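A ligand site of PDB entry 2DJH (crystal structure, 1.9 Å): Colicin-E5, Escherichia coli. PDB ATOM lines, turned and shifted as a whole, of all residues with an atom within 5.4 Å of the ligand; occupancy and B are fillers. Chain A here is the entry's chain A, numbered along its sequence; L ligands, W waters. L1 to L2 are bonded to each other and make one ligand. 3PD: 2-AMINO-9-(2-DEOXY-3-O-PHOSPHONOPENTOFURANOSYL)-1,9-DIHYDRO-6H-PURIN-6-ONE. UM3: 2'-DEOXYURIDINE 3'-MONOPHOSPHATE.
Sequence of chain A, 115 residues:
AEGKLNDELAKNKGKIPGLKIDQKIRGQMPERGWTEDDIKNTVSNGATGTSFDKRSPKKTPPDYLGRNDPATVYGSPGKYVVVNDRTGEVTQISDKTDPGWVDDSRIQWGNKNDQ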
ATOM      1  N   LYS A  24      -6.527  12.281 -11.429  1.00  0.00           N
ATOM      2  CA  LYS A  24      -7.104  12.620 -12.734  1.00  0.00           C
ATOM      3  C   LYS A  24      -6.019  12.644 -13.816  1.00  0.00           C
ATOM      4  O   LYS A  24      -6.149  11.993 -14.855  1.00  0.00           O
ATOM      5  CB  LYS A  24      -7.788  13.990 -12.630  1.00  0.00           C
ATOM      6  CG  LYS A  24      -9.125  14.087 -13.357  1.00  0.00           C
ATOM      7  CD  LYS A  24      -8.966  14.516 -14.805  1.00  0.00           C
ATOM      8  CE  LYS A  24     -10.182  15.303 -15.273  1.00  0.00           C
ATOM      9  NZ  LYS A  24      -9.915  16.760 -15.393  1.00  0.00           N
ATOM     10  N   GLN A  28      -4.888  10.075 -17.247  1.00  0.00           N
ATOM     11  CA  GLN A  28      -4.862  10.606 -18.598  1.00  0.00           C
ATOM     12  C   GLN A  28      -3.530  10.384 -19.298  1.00  0.00           C
ATOM     13  O   GLN A  28      -3.476  10.287 -20.515  1.00  0.00           O
ATOM     14  CB  GLN A  28      -5.163  12.110 -18.603  1.00  0.00           C
ATOM     15  CG  GLN A  28      -6.492  12.507 -17.986  1.00  0.00           C
ATOM     16  CD  GLN A  28      -6.720  14.007 -17.994  1.00  0.00           C
ATOM     17  OE1 GLN A  28      -5.781  14.789 -17.837  1.00  0.00           O
ATOM     18  NE2 GLN A  28      -7.967  14.412 -18.164  1.00  0.00           N
ATOM     19  N   ARG A  32      -2.927  10.052 -23.250  1.00  0.00           N
ATOM     20  CA  ARG A  32      -2.385  11.219 -23.939  1.00  0.00           C
ATOM     21  C   ARG A  32      -0.920  11.106 -24.322  1.00  0.00           C
ATOM     22  O   ARG A  32      -0.326  12.058 -24.802  1.00  0.00           O
ATOM     23  CB  ARG A  32      -2.631  12.473 -23.093  1.00  0.00           C
ATOM     24  CG  ARG A  32      -4.103  12.702 -22.783  1.00  0.00           C
ATOM     25  CD  ARG A  32      -4.398  14.062 -22.180  1.00  0.00           C
ATOM     26  NE  ARG A  32      -5.795  14.137 -21.759  1.00  0.00           N
ATOM     27  CZ  ARG A  32      -6.390  15.240 -21.309  1.00  0.00           C
ATOM     28  NH1 ARG A  32      -7.671  15.205 -20.952  1.00  0.00           N
ATOM     29  NH2 ARG A  32      -5.717  16.376 -21.214  1.00  0.00           N
ATOM     30  N   SER A  51       0.688  30.842 -18.127  1.00  0.00           N
ATOM     31  CA  SER A  51      -0.741  30.583 -18.240  1.00  0.00           C
ATOM     32  C   SER A  51      -1.398  30.843 -16.898  1.00  0.00           C
ATOM     33  O   SER A  51      -0.810  31.468 -16.023  1.00  0.00           O
ATOM     34  CB  SER A  51      -0.968  29.129 -18.672  1.00  0.00           C
ATOM     35  OG  SER A  51      -2.322  28.898 -19.004  1.00  0.00           O
ATOM     36  N   PHE A  52      -2.635  30.378 -16.756  1.00  0.00           N
ATOM     37  CA  PHE A  52      -3.361  30.527 -15.523  1.00  0.00           C
ATOM     38  C   PHE A  52      -4.099  29.227 -15.258  1.00  0.00           C
ATOM     39  O   PHE A  52      -4.686  28.649 -16.168  1.00  0.00           O
ATOM     40  CB  PHE A  52      -4.384  31.679 -15.602  1.00  0.00           C
ATOM     41  CG  PHE A  52      -3.747  33.034 -15.685  1.00  0.00           C
ATOM     42  CD1 PHE A  52      -3.599  33.670 -16.916  1.00  0.00           C
ATOM     43  CD2 PHE A  52      -3.270  33.658 -14.541  1.00  0.00           C
ATOM     44  CE1 PHE A  52      -2.977  34.907 -17.001  1.00  0.00           C
ATOM     45  CE2 PHE A  52      -2.634  34.898 -14.627  1.00  0.00           C
ATOM     46  CZ  PHE A  52      -2.490  35.523 -15.851  1.00  0.00           C
ATOM     47  N   ASP A  53      -4.024  28.752 -14.021  1.00  0.00           N
ATOM     48  CA  ASP A  53      -4.714  27.534 -13.622  1.00  0.00           C
ATOM     49  C   ASP A  53      -6.053  28.003 -13.051  1.00  0.00           C
ATOM     50  O   ASP A  53      -6.114  28.510 -11.939  1.00  0.00           O
ATOM     51  CB  ASP A  53      -3.902  26.781 -12.558  1.00  0.00           C
ATOM     52  CG  ASP A  53      -4.574  25.485 -12.118  1.00  0.00           C
ATOM     53  OD1 ASP A  53      -3.912  24.680 -11.432  1.00  0.00           O
ATOM     54  OD2 ASP A  53      -5.765  25.270 -12.450  1.00  0.00           O
ATOM     55  N   LYS A  54      -7.117  27.841 -13.842  1.00  0.00           N
ATOM     56  CA  LYS A  54      -8.454  28.250 -13.438  1.00  0.00           C
ATOM     57  C   LYS A  54      -9.378  27.032 -13.370  1.00  0.00           C
ATOM     58  O   LYS A  54     -10.572  27.124 -13.676  1.00  0.00           O
ATOM     59  CB  LYS A  54      -9.026  29.266 -14.436  1.00  0.00           C
ATOM     60  CG  LYS A  54      -8.165  30.510 -14.657  1.00  0.00           C
ATOM     61  CD  LYS A  54      -8.252  31.491 -13.501  1.00  0.00           C
ATOM     62  CE  LYS A  54      -9.632  32.124 -13.413  1.00  0.00           C
ATOM     63  NZ  LYS A  54      -9.967  32.924 -14.627  1.00  0.00           N
ATOM     64  N   ARG A  55      -8.813  25.894 -12.989  1.00  0.00           N
ATOM     65  CA  ARG A  55      -9.571  24.655 -12.893  1.00  0.00           C
ATOM     66  C   ARG A  55     -10.790  24.758 -11.988  1.00  0.00           C
ATOM     67  O   ARG A  55     -10.769  25.445 -10.959  1.00  0.00           O
ATOM     68  CB  ARG A  55      -8.677  23.514 -12.394  1.00  0.00           C
ATOM     69  CG  ARG A  55      -7.729  22.962 -13.446  1.00  0.00           C
ATOM     70  CD  ARG A  55      -6.874  21.842 -12.866  1.00  0.00           C
ATOM     71  NE  ARG A  55      -5.884  22.358 -11.929  1.00  0.00           N
ATOM     72  CZ  ARG A  55      -5.351  21.625 -10.951  1.00  0.00           C
ATOM     73  NH1 ARG A  55      -4.441  22.159 -10.136  1.00  0.00           N
ATOM     74  NH2 ARG A  55      -5.746  20.379 -10.767  1.00  0.00           N
ATOM     75  N   SER A  56     -11.855  24.070 -12.370  1.00  0.00           N
ATOM     76  CA  SER A  56     -13.094  24.050 -11.620  1.00  0.00           C
ATOM     77  C   SER A  56     -12.935  23.099 -10.438  1.00  0.00           C
ATOM     78  O   SER A  56     -12.053  22.232 -10.438  1.00  0.00           O
ATOM     79  CB  SER A  56     -14.248  23.583 -12.509  1.00  0.00           C
ATOM     80  OG  SER A  56     -13.994  22.276 -12.996  1.00  0.00           O
ATOM     81  N   LYS A  58     -14.470  20.363  -9.342  1.00  0.00           N
ATOM     82  CA  LYS A  58     -14.448  18.933  -9.621  1.00  0.00           C
ATOM     83  C   LYS A  58     -13.088  18.406 -10.088  1.00  0.00           C
ATOM     84  O   LYS A  58     -12.788  17.230  -9.906  1.00  0.00           O
ATOM     85  CB  LYS A  58     -15.515  18.583 -10.662  1.00  0.00           C
ATOM     86  CG  LYS A  58     -15.305  19.205 -12.019  1.00  0.00           C
ATOM     87  CD  LYS A  58     -16.538  19.018 -12.901  1.00  0.00           C
ATOM     88  CE  LYS A  58     -16.303  19.519 -14.311  1.00  0.00           C
ATOM     89  NZ  LYS A  58     -15.308  18.686 -15.037  1.00  0.00           N
ATOM     90  N   LYS A  59     -12.264  19.283 -10.659  1.00  0.00           N
ATOM     91  CA  LYS A  59     -10.962  18.860 -11.151  1.00  0.00           C
ATOM     92  C   LYS A  59      -9.758  19.265 -10.317  1.00  0.00           C
ATOM     93  O   LYS A  59      -8.627  19.290 -10.828  1.00  0.00           O
ATOM     94  CB  LYS A  59     -10.783  19.336 -12.594  1.00  0.00           C
ATOM     95  CG  LYS A  59     -11.796  18.739 -13.549  1.00  0.00           C
ATOM     96  CD  LYS A  59     -11.529  19.095 -14.990  1.00  0.00           C
ATOM     97  CE  LYS A  59     -12.494  18.371 -15.906  1.00  0.00           C
ATOM     98  NZ  LYS A  59     -12.335  18.778 -17.320  1.00  0.00           N
ATOM     99  N   TYR A  80       2.432  19.807 -24.454  1.00  0.00           N
ATOM    100  CA  TYR A  80       2.851  20.594 -23.310  1.00  0.00           C
ATOM    101  C   TYR A  80       2.343  20.136 -21.945  1.00  0.00           C
ATOM    102  O   TYR A  80       1.464  19.286 -21.835  1.00  0.00           O
ATOM    103  CB  TYR A  80       2.438  22.057 -23.509  1.00  0.00           C
ATOM    104  CG  TYR A  80       0.932  22.265 -23.594  1.00  0.00           C
ATOM    105  CD1 TYR A  80       0.282  22.419 -24.819  1.00  0.00           C
ATOM    106  CD2 TYR A  80       0.157  22.291 -22.435  1.00  0.00           C
ATOM    107  CE1 TYR A  80      -1.100  22.590 -24.886  1.00  0.00           C
ATOM    108  CE2 TYR A  80      -1.223  22.459 -22.493  1.00  0.00           C
ATOM    109  CZ  TYR A  80      -1.837  22.609 -23.715  1.00  0.00           C
ATOM    110  OH  TYR A  80      -3.201  22.775 -23.765  1.00  0.00           O
ATOM    111  N   VAL A  82       1.313  22.057 -18.183  1.00  0.00           N
ATOM    112  CA  VAL A  82       1.054  23.308 -17.478  1.00  0.00           C
ATOM    113  C   VAL A  82       1.170  23.017 -15.988  1.00  0.00           C
ATOM    114  O   VAL A  82       0.595  22.047 -15.497  1.00  0.00           O
ATOM    115  CB  VAL A  82      -0.343  23.869 -17.788  1.00  0.00           C
ATOM    116  CG1 VAL A  82      -0.559  25.180 -17.044  1.00  0.00           C
ATOM    117  CG2 VAL A  82      -0.502  24.077 -19.282  1.00  0.00           C
ATOM    118  N   THR A  91      -1.396  21.158 -13.934  1.00  0.00           N
ATOM    119  CA  THR A  91      -2.734  21.648 -14.294  1.00  0.00           C
ATOM    120  C   THR A  91      -3.302  20.870 -15.474  1.00  0.00           C
ATOM    121  O   THR A  91      -4.491  20.530 -15.497  1.00  0.00           O
ATOM    122  CB  THR A  91      -2.686  23.141 -14.680  1.00  0.00           C
ATOM    123  OG1 THR A  91      -2.070  23.873 -13.613  1.00  0.00           O
ATOM    124  CG2 THR A  91      -4.102  23.683 -14.918  1.00  0.00           C
ATOM    125  N   GLN A  92      -2.461  20.617 -16.463  1.00  0.00           N
ATOM    126  CA  GLN A  92      -2.894  19.891 -17.646  1.00  0.00           C
ATOM    127  C   GLN A  92      -1.734  19.340 -18.449  1.00  0.00           C
ATOM    128  O   GLN A  92      -0.621  19.862 -18.405  1.00  0.00           O
ATOM    129  CB  GLN A  92      -3.728  20.812 -18.550  1.00  0.00           C
ATOM    130  CG  GLN A  92      -3.954  20.288 -19.970  1.00  0.00           C
ATOM    131  CD  GLN A  92      -4.820  21.207 -20.826  1.00  0.00           C
ATOM    132  OE1 GLN A  92      -6.031  21.006 -20.964  1.00  0.00           O
ATOM    133  NE2 GLN A  92      -4.197  22.228 -21.403  1.00  0.00           N
ATOM    134  N   ILE A  93      -2.000  18.263 -19.158  1.00  0.00           N
ATOM    135  CA  ILE A  93      -1.030  17.669 -20.067  1.00  0.00           C
ATOM    136  C   ILE A  93      -1.846  17.552 -21.352  1.00  0.00           C
ATOM    137  O   ILE A  93      -2.961  17.030 -21.341  1.00  0.00           O
ATOM    138  CB  ILE A  93      -0.526  16.273 -19.615  1.00  0.00           C
ATOM    139  CG1 ILE A  93      -1.706  15.347 -19.320  1.00  0.00           C
ATOM    140  CG2 ILE A  93       0.385  16.424 -18.398  1.00  0.00           C
ATOM    141  CD1 ILE A  93      -1.293  13.917 -19.053  1.00  0.00           C
ATOM    142  N   ASP A  98      -3.312  13.477 -30.272  1.00  0.00           N
ATOM    143  CA  ASP A  98      -4.327  14.209 -31.015  1.00  0.00           C
ATOM    144  C   ASP A  98      -3.690  15.347 -31.820  1.00  0.00           C
ATOM    145  O   ASP A  98      -3.326  16.391 -31.273  1.00  0.00           O
ATOM    146  CB  ASP A  98      -5.365  14.783 -30.026  1.00  0.00           C
ATOM    147  CG  ASP A  98      -6.477  15.553 -30.726  1.00  0.00           C
ATOM    148  OD1 ASP A  98      -6.429  15.711 -31.960  1.00  0.00           O
ATOM    149  OD2 ASP A  98      -7.412  16.008 -30.022  1.00  0.00           O
ATOM    150  N   GLY A 100      -5.067  17.321 -33.713  1.00  0.00           N
ATOM    151  CA  GLY A 100      -5.957  18.478 -33.758  1.00  0.00           C
ATOM    152  C   GLY A 100      -6.081  19.179 -32.414  1.00  0.00           C
ATOM    153  O   GLY A 100      -6.957  20.019 -32.241  1.00  0.00           O
ATOM    154  N   TRP A 101      -5.209  18.852 -31.472  1.00  0.00           N
ATOM    155  CA  TRP A 101      -5.286  19.481 -30.144  1.00  0.00           C
ATOM    156  C   TRP A 101      -5.161  21.003 -30.192  1.00  0.00           C
ATOM    157  O   TRP A 101      -4.227  21.551 -30.773  1.00  0.00           O
ATOM    158  CB  TRP A 101      -4.201  18.892 -29.224  1.00  0.00           C
ATOM    159  CG  TRP A 101      -4.262  19.406 -27.803  1.00  0.00           C
ATOM    160  CD1 TRP A 101      -3.641  20.523 -27.303  1.00  0.00           C
ATOM    161  CD2 TRP A 101      -4.998  18.836 -26.707  1.00  0.00           C
ATOM    162  NE1 TRP A 101      -3.939  20.674 -25.967  1.00  0.00           N
ATOM    163  CE2 TRP A 101      -4.773  19.647 -25.575  1.00  0.00           C
ATOM    164  CE3 TRP A 101      -5.833  17.715 -26.583  1.00  0.00           C
ATOM    165  CZ2 TRP A 101      -5.349  19.377 -24.330  1.00  0.00           C
ATOM    166  CZ3 TRP A 101      -6.401  17.440 -25.341  1.00  0.00           C
ATOM    167  CH2 TRP A 101      -6.153  18.276 -24.225  1.00  0.00           C
ATOM    168  N   VAL A 102      -6.132  21.682 -29.587  1.00  0.00           N
ATOM    169  CA  VAL A 102      -6.128  23.138 -29.522  1.00  0.00           C
ATOM    170  C   VAL A 102      -5.629  23.537 -28.134  1.00  0.00           C
ATOM    171  O   VAL A 102      -6.214  23.159 -27.128  1.00  0.00           O
ATOM    172  CB  VAL A 102      -7.558  23.705 -29.714  1.00  0.00           C
ATOM    173  CG1 VAL A 102      -7.485  25.218 -29.867  1.00  0.00           C
ATOM    174  CG2 VAL A 102      -8.234  23.070 -30.917  1.00  0.00           C
ATOM    175  N   ASP A 103      -4.537  24.296 -28.088  1.00  0.00           N
ATOM    176  CA  ASP A 103      -3.975  24.726 -26.807  1.00  0.00           C
ATOM    177  C   ASP A 103      -5.013  25.428 -25.953  1.00  0.00           C
ATOM    178  O   ASP A 103      -5.886  26.130 -26.470  1.00  0.00           O
ATOM    179  CB  ASP A 103      -2.793  25.672 -27.040  1.00  0.00           C
ATOM    180  CG  ASP A 103      -1.641  25.013 -27.755  1.00  0.00           C
ATOM    181  OD1 ASP A 103      -1.647  23.771 -27.886  1.00  0.00           O
ATOM    182  OD2 ASP A 103      -0.716  25.732 -28.178  1.00  0.00           O
ATOM    183  N   ASP A 104      -4.933  25.241 -24.644  1.00  0.00           N
ATOM    184  CA  ASP A 104      -5.876  25.882 -23.742  1.00  0.00           C
ATOM    185  C   ASP A 104      -5.810  27.395 -23.970  1.00  0.00           C
ATOM    186  O   ASP A 104      -4.737  27.925 -24.265  1.00  0.00           O
ATOM    187  CB  ASP A 104      -5.546  25.541 -22.298  1.00  0.00           C
ATOM    188  CG  ASP A 104      -6.535  26.158 -21.322  1.00  0.00           C
ATOM    189  OD1 ASP A 104      -6.285  27.303 -20.867  1.00  0.00           O
ATOM    190  OD2 ASP A 104      -7.548  25.512 -21.007  1.00  0.00           O
ATOM    191  N   ARG A 106      -5.781  29.891 -22.000  1.00  0.00           N
ATOM    192  CA  ARG A 106      -5.005  30.705 -21.070  1.00  0.00           C
ATOM    193  C   ARG A 106      -3.508  30.706 -21.347  1.00  0.00           C
ATOM    194  O   ARG A 106      -2.790  31.546 -20.822  1.00  0.00           O
ATOM    195  CB  ARG A 106      -5.285  30.259 -19.641  1.00  0.00           C
ATOM    196  CG  ARG A 106      -6.602  30.767 -19.134  1.00  0.00           C
ATOM    197  CD  ARG A 106      -7.278  29.791 -18.192  1.00  0.00           C
ATOM    198  NE  ARG A 106      -7.676  28.581 -18.888  1.00  0.00           N
ATOM    199  CZ  ARG A 106      -8.900  28.048 -18.819  1.00  0.00           C
ATOM    200  NH1 ARG A 106      -9.832  28.630 -18.064  1.00  0.00           N
ATOM    201  NH2 ARG A 106      -9.178  26.943 -19.483  1.00  0.00           N
ATOM    202  N   ILE A 107      -3.050  29.791 -22.189  1.00  0.00           N
ATOM    203  CA  ILE A 107      -1.637  29.684 -22.495  1.00  0.00           C
ATOM    204  C   ILE A 107      -1.107  30.829 -23.355  1.00  0.00           C
ATOM    205  O   ILE A 107      -1.683  31.184 -24.391  1.00  0.00           O
ATOM    206  CB  ILE A 107      -1.325  28.340 -23.203  1.00  0.00           C
ATOM    207  CG1 ILE A 107      -1.604  27.188 -22.224  1.00  0.00           C
ATOM    208  CG2 ILE A 107       0.120  28.290 -23.666  1.00  0.00           C
ATOM    209  CD1 ILE A 107      -1.563  25.825 -22.850  1.00  0.00           C
HETATM  210  O5' 3PD L   1     -10.442  22.117 -22.351  1.00  0.00           O
HETATM  211  C5' 3PD L   1     -11.268  21.448 -21.400  1.00  0.00           C
HETATM  212  C4' 3PD L   1     -11.105  19.945 -21.480  1.00  0.00           C
HETATM  213  O4' 3PD L   1     -11.540  19.406 -22.772  1.00  0.00           O
HETATM  214  C1' 3PD L   1     -10.758  18.305 -23.145  1.00  0.00           C
HETATM  215  C2' 3PD L   1      -9.680  18.067 -22.070  1.00  0.00           C
HETATM  216  C3' 3PD L   1      -9.662  19.421 -21.294  1.00  0.00           C
HETATM  217  O3' 3PD L   1      -9.452  19.257 -19.867  1.00  0.00           O
HETATM  218  N9  3PD L   1     -10.248  18.529 -24.561  1.00  0.00           N
HETATM  219  C4  3PD L   1      -9.380  19.518 -25.051  1.00  0.00           C
HETATM  220  N3  3PD L   1      -8.797  20.543 -24.297  1.00  0.00           N
HETATM  221  C2  3PD L   1      -7.993  21.363 -25.030  1.00  0.00           C
HETATM  222  N2  3PD L   1      -7.341  22.386 -24.463  1.00  0.00           N
HETATM  223  N1  3PD L   1      -7.787  21.178 -26.407  1.00  0.00           N
HETATM  224  C6  3PD L   1      -8.390  20.128 -27.201  1.00  0.00           C
HETATM  225  O6  3PD L   1      -8.140  20.068 -28.404  1.00  0.00           O
HETATM  226  C5  3PD L   1      -9.240  19.266 -26.422  1.00  0.00           C
HETATM  227  N7  3PD L   1      -9.981  18.157 -26.800  1.00  0.00           N
HETATM  228  C8  3PD L   1     -10.545  17.759 -25.686  1.00  0.00           C
HETATM  229  P   3PD L   1      -8.270  18.403 -19.202  1.00  0.00           P
HETATM  230  O1P 3PD L   1      -8.793  17.087 -18.828  1.00  0.00           O
HETATM  231  O2P 3PD L   1      -7.087  18.416 -20.098  1.00  0.00           O
HETATM  232  N1  UM3 L   2      -6.524  24.420 -17.604  1.00  0.00           N
HETATM  233  C2  UM3 L   2      -6.236  25.696 -17.026  1.00  0.00           C
HETATM  234  N3  UM3 L   2      -5.097  26.332 -17.563  1.00  0.00           N
HETATM  235  C4  UM3 L   2      -4.266  25.848 -18.578  1.00  0.00           C
HETATM  236  C5  UM3 L   2      -4.633  24.546 -19.121  1.00  0.00           C
HETATM  237  C6  UM3 L   2      -5.727  23.877 -18.637  1.00  0.00           C
HETATM  238  O2  UM3 L   2      -6.901  26.201 -16.129  1.00  0.00           O
HETATM  239  O4  UM3 L   2      -3.306  26.522 -18.938  1.00  0.00           O
HETATM  240  C1' UM3 L   2      -7.751  23.707 -17.007  1.00  0.00           C
HETATM  241  C2' UM3 L   2      -8.930  23.369 -17.916  1.00  0.00           C
HETATM  242  C3' UM3 L   2      -9.402  22.017 -17.314  1.00  0.00           C
HETATM  243  C4' UM3 L   2      -8.061  21.381 -16.904  1.00  0.00           C
HETATM  244  O3' UM3 L   2     -10.171  22.189 -16.096  1.00  0.00           O
HETATM  245  O4' UM3 L   2      -7.266  22.505 -16.452  1.00  0.00           O
HETATM  246  C5' UM3 L   2      -7.386  20.550 -17.957  1.00  0.00           C
HETATM  247  O5' UM3 L   2      -7.942  19.223 -17.876  1.00  0.00           O
HETATM  248  P   UM3 L   2     -11.594  22.761 -16.278  1.00  0.00           P
HETATM  249  O1P UM3 L   2     -12.194  22.847 -14.982  1.00  0.00           O
HETATM  250  O2P UM3 L   2     -12.355  21.882 -17.106  1.00  0.00           O
HETATM  251  O3P UM3 L   2     -11.583  24.086 -16.845  1.00  0.00           O
HETATM  252  O   HOH W   1     -11.276  16.063 -18.831  1.00  0.00           O
HETATM  253  O   HOH W   2     -12.251  26.358 -15.580  1.00  0.00           O
HETATM  254  O   HOH W   3     -14.981  21.486 -16.633  1.00  0.00           O
HETATM  255  O   HOH W   4      -4.801  17.330 -18.306  1.00  0.00           O
HETATM  256  O   HOH W   5      -7.877  22.935 -21.735  1.00  0.00           O
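Water W2 bridges the backbone carbonyl oxygen of Lys 54 (2.7 Å) and an oxygen (O3P) of UM3 L2 (2.7 Å).
Water W1 bridges O1P of 3PD L1 (2.7 Å) and NZ of Lys 59 (3.3 Å).
Water W3 bridges O2P of UM3 L2 and NZ of Lys 58.
Water W5 lies within hydrogen-bond range of OD2 of Asp 104 (2.7 Å), O5' of 3PD L1 (2.8 Å) and OE1 of Gln 92 (2.8 Å).
Water W4 lies within hydrogen-bond range of the side-chain amide oxygen (OE1) of Gln 28 (2.8 Å), the backbone NH (N) of Ile 93 (3.1 Å), an oxygen (O2P) of 3PD L1 (3.1 Å) and the guanidinium group (NH2) of Arg 32 (3.2 Å).
The side-chain carboxylate (OD1) of Asp 98 sits at hydrogen-bond distance from the backbone NH (N) of Trp 101, at 3.4 Å.
OG1 of Thr 91 sits at hydrogen-bond distance from OD1 of Asp 53.
The guanidinium group (NH2) of Arg 32 lies within hydrogen-bond range of the backbone carbonyl oxygen (O) of Ile 93.
NH1 of Arg 55 lies within salt-bridge range of OD1 of Asp 53 (2.9 Å).
The side-chain hydroxyl (OH) of Tyr 80 lies within hydrogen-bond range of the backbone NH (N) of Asp 104 (3.1 Å).
The backbone NH of Thr 91 is in hydrogen-bond range of the backbone carbonyl oxygen of Val 82, 2.7 Å away.
The guanidinium group (NH1) of Arg 32 sits close to the side-chain amide nitrogen (NE2) of Gln 28 (2.9 Å).
The side-chain hydroxyl (OG) of Ser 51 lies within hydrogen-bond range of the backbone NH (N) of Ile 107 (3.4 Å).
Lys 24 touches the ligand.
CA of Asp 53 touches O2 of UM3 L2 (3.6 Å).
CG of Arg 55 touches O4' of UM3 L2 (3.1 Å).
CG1 of Val 82 touches O4 of UM3 L2, at 3.6 Å.
O of Thr 91 touches O4' of UM3 L2 (3.5 Å).
Trp 101 touches the ligand.
CG of Asp 104 touches C5 of UM3 L2 (3.3 Å).
NE of Arg 106 touches N3 of UM3 L2, 3.7 Å away.
Ile 107 touches the ligand.
The nearest printed residue that does not touch the ligand is Gly 100 (4.02 Å).
An oxygen (O2P) of 3PD L1 sits at hydrogen-bond distance from the side-chain amide oxygen of Gln 92 (2.9 Å).
The backbone NH (N) of Val 102 is in hydrogen-bond range of an oxygen (O6) of 3PD L1 (2.8 Å).
O2 of UM3 L2 lies within hydrogen-bond range of N of Lys 54 (2.8 Å).
An oxygen (O1P) of 3PD L1 is in hydrogen-bond range of the side-chain amide nitrogen (NE2) of Gln 28 (2.9 Å).
OG of Ser 51 sits at hydrogen-bond distance from O4 of UM3 L2 (2.6 Å).
OG of Ser 56 lies within hydrogen-bond range of O1P of UM3 L2 (2.7 Å).
The backbone carbonyl oxygen of Phe 52 lies within hydrogen-bond range of a nitrogen (N3) of UM3 L2, at 2.7 Å.
A nitrogen (N1) of 3PD L1 sits at hydrogen-bond distance from the backbone carbonyl oxygen (O) of Val 102.
The side-chain amino group (NZ) of Lys 59 lies within salt-bridge range of an oxygen (O2P) of UM3 L2, 3.1 Å away.
O2P of 3PD L1 sits at hydrogen-bond distance from NH2 of Arg 32 (2.7 Å).
N of Ser 56 lies within hydrogen-bond range of O1P of UM3 L2, at 2.9 Å.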
